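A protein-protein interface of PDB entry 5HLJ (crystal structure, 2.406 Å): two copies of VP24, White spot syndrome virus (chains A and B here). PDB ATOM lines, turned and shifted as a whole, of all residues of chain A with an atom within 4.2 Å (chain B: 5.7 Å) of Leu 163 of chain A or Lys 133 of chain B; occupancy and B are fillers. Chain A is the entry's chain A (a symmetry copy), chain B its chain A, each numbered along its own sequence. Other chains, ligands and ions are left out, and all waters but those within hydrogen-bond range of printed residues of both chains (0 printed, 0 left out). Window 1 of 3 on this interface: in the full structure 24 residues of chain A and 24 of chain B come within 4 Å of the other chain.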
ATOM      1  N   LEU A  23      20.484   6.884  -8.328  1.00  0.00           N
ATOM      2  CA  LEU A  23      21.319   6.242  -9.335  1.00  0.00           C
ATOM      3  C   LEU A  23      21.834   4.889  -8.850  1.00  0.00           C
ATOM      4  O   LEU A  23      21.820   4.590  -7.654  1.00  0.00           O
ATOM      5  CB  LEU A  23      22.512   7.129  -9.689  1.00  0.00           C
ATOM      6  CG  LEU A  23      22.226   8.521 -10.246  1.00  0.00           C
ATOM      7  CD1 LEU A  23      23.534   9.207 -10.540  1.00  0.00           C
ATOM      8  CD2 LEU A  23      21.360   8.432 -11.506  1.00  0.00           C
ATOM      9  N   THR A  24      22.326   4.088  -9.785  1.00  0.00           N
ATOM     10  CA  THR A  24      22.898   2.794  -9.456  1.00  0.00           C
ATOM     11  C   THR A  24      24.419   2.828  -9.585  1.00  0.00           C
ATOM     12  O   THR A  24      24.944   3.447 -10.501  1.00  0.00           O
ATOM     13  CB  THR A  24      22.290   1.702 -10.357  1.00  0.00           C
ATOM     14  OG1 THR A  24      20.888   1.616 -10.082  1.00  0.00           O
ATOM     15  CG2 THR A  24      22.900   0.368 -10.068  1.00  0.00           C
ATOM     16  N   SER A 111      23.266   9.046   0.368  1.00  0.00           N
ATOM     17  CA  SER A 111      23.102   7.833   1.145  1.00  0.00           C
ATOM     18  C   SER A 111      23.189   6.645   0.209  1.00  0.00           C
ATOM     19  O   SER A 111      23.042   6.788  -1.002  1.00  0.00           O
ATOM     20  CB  SER A 111      21.783   7.843   1.934  1.00  0.00           C
ATOM     21  OG  SER A 111      20.681   8.106   1.094  1.00  0.00           O
ATOM     22  N   LEU A 112      23.477   5.483   0.781  1.00  0.00           N
ATOM     23  CA  LEU A 112      23.643   4.257   0.029  1.00  0.00           C
ATOM     24  C   LEU A 112      22.773   3.168   0.595  1.00  0.00           C
ATOM     25  O   LEU A 112      22.599   3.052   1.806  1.00  0.00           O
ATOM     26  CB  LEU A 112      25.091   3.746   0.069  1.00  0.00           C
ATOM     27  CG  LEU A 112      26.267   4.342  -0.687  1.00  0.00           C
ATOM     28  CD1 LEU A 112      27.436   3.408  -0.441  1.00  0.00           C
ATOM     29  CD2 LEU A 112      25.994   4.484  -2.181  1.00  0.00           C
ATOM     30  N   SER A 113      22.276   2.337  -0.299  1.00  0.00           N
ATOM     31  CA  SER A 113      21.683   1.083   0.073  1.00  0.00           C
ATOM     32  C   SER A 113      22.356   0.020  -0.787  1.00  0.00           C
ATOM     33  O   SER A 113      22.604   0.262  -1.967  1.00  0.00           O
ATOM     34  CB  SER A 113      20.171   1.113  -0.152  1.00  0.00           C
ATOM     35  OG  SER A 113      19.629  -0.201  -0.162  1.00  0.00           O
ATOM     36  N   TYR A 162      25.290  -1.358  -5.432  1.00  0.00           N
ATOM     37  CA  TYR A 162      24.724  -0.348  -4.538  1.00  0.00           C
ATOM     38  C   TYR A 162      23.784   0.628  -5.236  1.00  0.00           C
ATOM     39  O   TYR A 162      23.861   0.838  -6.448  1.00  0.00           O
ATOM     40  CB  TYR A 162      25.850   0.424  -3.820  1.00  0.00           C
ATOM     41  CG  TYR A 162      26.395  -0.414  -2.699  1.00  0.00           C
ATOM     42  CD1 TYR A 162      27.379  -1.396  -2.931  1.00  0.00           C
ATOM     43  CD2 TYR A 162      25.889  -0.286  -1.417  1.00  0.00           C
ATOM     44  CE1 TYR A 162      27.843  -2.214  -1.892  1.00  0.00           C
ATOM     45  CE2 TYR A 162      26.340  -1.085  -0.389  1.00  0.00           C
ATOM     46  CZ  TYR A 162      27.314  -2.048  -0.625  1.00  0.00           C
ATOM     47  OH  TYR A 162      27.731  -2.819   0.433  1.00  0.00           O
ATOM     48  N   LEU A 163      22.882   1.198  -4.440  1.00  0.00           N
ATOM     49  CA  LEU A 163      21.946   2.224  -4.889  1.00  0.00           C
ATOM     50  C   LEU A 163      22.348   3.518  -4.230  1.00  0.00           C
ATOM     51  O   LEU A 163      22.558   3.559  -3.022  1.00  0.00           O
ATOM     52  CB  LEU A 163      20.510   1.859  -4.527  1.00  0.00           C
ATOM     53  CG  LEU A 163      20.101   0.436  -4.916  1.00  0.00           C
ATOM     54  CD1 LEU A 163      18.705   0.068  -4.390  1.00  0.00           C
ATOM     55  CD2 LEU A 163      20.163   0.321  -6.432  1.00  0.00           C
ATOM     56  N   LEU A 164      22.473   4.569  -5.027  1.00  0.00           N
ATOM     57  CA  LEU A 164      22.976   5.837  -4.541  1.00  0.00           C
ATOM     58  C   LEU A 164      21.878   6.892  -4.545  1.00  0.00           C
ATOM     59  O   LEU A 164      21.227   7.111  -5.559  1.00  0.00           O
ATOM     60  CB  LEU A 164      24.152   6.291  -5.411  1.00  0.00           C
ATOM     61  CG  LEU A 164      24.703   7.715  -5.231  1.00  0.00           C
ATOM     62  CD1 LEU A 164      25.390   7.884  -3.873  1.00  0.00           C
ATOM     63  CD2 LEU A 164      25.665   8.068  -6.377  1.00  0.00           C
ATOM     64  N   SER A 165      21.669   7.534  -3.406  1.00  0.00           N
ATOM     65  CA  SER A 165      20.769   8.670  -3.334  1.00  0.00           C
ATOM     66  C   SER A 165      21.543   9.960  -3.135  1.00  0.00           C
ATOM     67  O   SER A 165      22.326  10.074  -2.197  1.00  0.00           O
ATOM     68  CB  SER A 165      19.757   8.505  -2.202  1.00  0.00           C
ATOM     69  OG  SER A 165      18.717   7.627  -2.569  1.00  0.00           O
ATOM     70  N   VAL B 107       8.411   6.881  -3.367  1.00  0.00           N
ATOM     71  CA  VAL B 107       9.122   6.852  -2.101  1.00  0.00           C
ATOM     72  C   VAL B 107      10.615   6.775  -2.422  1.00  0.00           C
ATOM     73  O   VAL B 107      11.098   5.755  -2.896  1.00  0.00           O
ATOM     74  CB  VAL B 107       8.667   5.677  -1.207  1.00  0.00           C
ATOM     75  CG1 VAL B 107       9.326   5.758   0.170  1.00  0.00           C
ATOM     76  CG2 VAL B 107       7.153   5.712  -1.049  1.00  0.00           C
ATOM     77  N   ASP B 108      11.319   7.882  -2.183  1.00  0.00           N
ATOM     78  CA  ASP B 108      12.707   8.070  -2.614  1.00  0.00           C
ATOM     79  C   ASP B 108      13.716   7.365  -1.750  1.00  0.00           C
ATOM     80  O   ASP B 108      14.707   6.829  -2.245  1.00  0.00           O
ATOM     81  CB  ASP B 108      13.064   9.553  -2.612  1.00  0.00           C
ATOM     82  CG  ASP B 108      12.419  10.302  -3.717  1.00  0.00           C
ATOM     83  OD1 ASP B 108      12.521   9.847  -4.879  1.00  0.00           O
ATOM     84  OD2 ASP B 108      11.800  11.345  -3.420  1.00  0.00           O
ATOM     85  N   TYR B 131      18.205  -1.944   3.749  1.00  0.00           N
ATOM     86  CA  TYR B 131      17.961  -2.134   2.334  1.00  0.00           C
ATOM     87  C   TYR B 131      16.719  -1.342   1.886  1.00  0.00           C
ATOM     88  O   TYR B 131      15.636  -1.488   2.458  1.00  0.00           O
ATOM     89  CB  TYR B 131      17.784  -3.623   1.976  1.00  0.00           C
ATOM     90  CG  TYR B 131      17.240  -3.780   0.569  1.00  0.00           C
ATOM     91  CD1 TYR B 131      18.056  -3.586  -0.532  1.00  0.00           C
ATOM     92  CD2 TYR B 131      15.894  -4.045   0.344  1.00  0.00           C
ATOM     93  CE1 TYR B 131      17.555  -3.680  -1.821  1.00  0.00           C
ATOM     94  CE2 TYR B 131      15.381  -4.126  -0.940  1.00  0.00           C
ATOM     95  CZ  TYR B 131      16.220  -3.949  -2.012  1.00  0.00           C
ATOM     96  OH  TYR B 131      15.735  -4.045  -3.285  1.00  0.00           O
ATOM     97  N   PHE B 132      16.872  -0.511   0.857  1.00  0.00           N
ATOM     98  CA  PHE B 132      15.714   0.131   0.252  1.00  0.00           C
ATOM     99  C   PHE B 132      15.935   0.521  -1.202  1.00  0.00           C
ATOM    100  O   PHE B 132      16.910   1.186  -1.540  1.00  0.00           O
ATOM    101  CB  PHE B 132      15.289   1.392   1.029  1.00  0.00           C
ATOM    102  CG  PHE B 132      14.044   2.031   0.465  1.00  0.00           C
ATOM    103  CD1 PHE B 132      12.806   1.404   0.600  1.00  0.00           C
ATOM    104  CD2 PHE B 132      14.113   3.212  -0.254  1.00  0.00           C
ATOM    105  CE1 PHE B 132      11.653   1.967   0.070  1.00  0.00           C
ATOM    106  CE2 PHE B 132      12.964   3.789  -0.788  1.00  0.00           C
ATOM    107  CZ  PHE B 132      11.727   3.160  -0.618  1.00  0.00           C
ATOM    108  N   LYS B 133      14.986   0.134  -2.045  1.00  0.00           N
ATOM    109  CA  LYS B 133      14.953   0.513  -3.458  1.00  0.00           C
ATOM    110  C   LYS B 133      13.787   1.480  -3.703  1.00  0.00           C
ATOM    111  O   LYS B 133      12.667   1.214  -3.257  1.00  0.00           O
ATOM    112  CB  LYS B 133      14.817  -0.752  -4.304  1.00  0.00           C
ATOM    113  CG  LYS B 133      14.413  -0.578  -5.757  1.00  0.00           C
ATOM    114  CD  LYS B 133      14.318  -1.979  -6.387  1.00  0.00           C
ATOM    115  CE  LYS B 133      13.666  -1.995  -7.755  1.00  0.00           C
ATOM    116  NZ  LYS B 133      14.513  -1.347  -8.775  1.00  0.00           N
ATOM    117  N   PRO B 134      14.045   2.615  -4.381  1.00  0.00           N
ATOM    118  CA  PRO B 134      12.959   3.574  -4.641  1.00  0.00           C
ATOM    119  C   PRO B 134      11.739   2.887  -5.252  1.00  0.00           C
ATOM    120  O   PRO B 134      11.895   2.046  -6.122  1.00  0.00           O
ATOM    121  CB  PRO B 134      13.586   4.567  -5.626  1.00  0.00           C
ATOM    122  CG  PRO B 134      15.062   4.501  -5.312  1.00  0.00           C
ATOM    123  CD  PRO B 134      15.333   3.071  -4.933  1.00  0.00           C
ATOM    124  N   THR B 135      10.552   3.244  -4.772  1.00  0.00           N
ATOM    125  CA  THR B 135       9.319   2.541  -5.089  1.00  0.00           C
ATOM    126  C   THR B 135       8.216   3.501  -5.476  1.00  0.00           C
ATOM    127  O   THR B 135       7.902   4.421  -4.711  1.00  0.00           O
ATOM    128  CB  THR B 135       8.815   1.731  -3.891  1.00  0.00           C
ATOM    129  OG1 THR B 135       9.806   0.774  -3.496  1.00  0.00           O
ATOM    130  CG2 THR B 135       7.490   1.037  -4.232  1.00  0.00           C
ATOM    131  N   VAL B 146       8.408  -2.141   0.513  1.00  0.00           N
ATOM    132  CA  VAL B 146       9.234  -2.901   1.441  1.00  0.00           C
ATOM    133  C   VAL B 146      10.569  -2.215   1.723  1.00  0.00           C
ATOM    134  O   VAL B 146      11.098  -1.466   0.899  1.00  0.00           O
ATOM    135  CB  VAL B 146       9.528  -4.368   0.922  1.00  0.00           C
ATOM    136  CG1 VAL B 146       8.316  -4.991   0.245  1.00  0.00           C
ATOM    137  CG2 VAL B 146      10.707  -4.411  -0.009  1.00  0.00           C
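Among the printed residues, pairs that only touch across the chains: Ser 113 of chain A with Tyr 131 of chain B (3.6 Å), Leu 163 of chain A with Phe 132 of chain B (3.5 Å) and Leu 163 of chain A with Lys 133 of chain B (3.9 Å).
The backbone carbonyl oxygen of Lys 133 of chain B is in hydrogen-bond range of the side-chain hydroxyl of Thr 135 of chain B.
N of Leu 163 of chain A is in hydrogen-bond range of O of Ser 113 of chain A (2.7 Å).
Hydrophobic or aromatic side chains of chain A that line the printed part of chain B: Leu 163.
Of the 8 printed residues of chain B, 3 touch a printed residue of chain A.
Among the printed residues, 4 pairs touch across the chains.
Among the printed residues, no Asp or Glu carboxylate lies within 4 Å of a Lys or Arg side-chain nitrogen of the other chain.
No position is printed for both chains.
Of the printed residues of chain B, Ser 113 of chain A touches Tyr 131 (3.6 Å) and Phe 132 (3.0 Å).
Leu 164 of chain A touches none of the printed residues of chain B.
Printed residues of chain A within 4 Å of Tyr 131 of chain B: Ser 113.
Of the printed residues of chain A, Phe 132 of chain B touches Ser 113 (3.0 Å) and Leu 163 (3.5 Å).
Of the printed residues of chain A, Lys 133 of chain B touches Leu 163.
Thr 135 of chain B touches none of the printed residues of chain A.
The nearest residue of chain B that does not touch Leu 163 of chain A is Pro 134 of chain B (4.5 Å).
The nearest printed residue of chain A that does not touch Phe 132 of chain B is Leu 112 of chain A (6.5 Å).
The side-chain hydroxyl (OG) of Ser 113 of chain A sits at hydrogen-bond distance from the backbone NH (N) of Phe 132 of chain B, at 3.0 Å.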
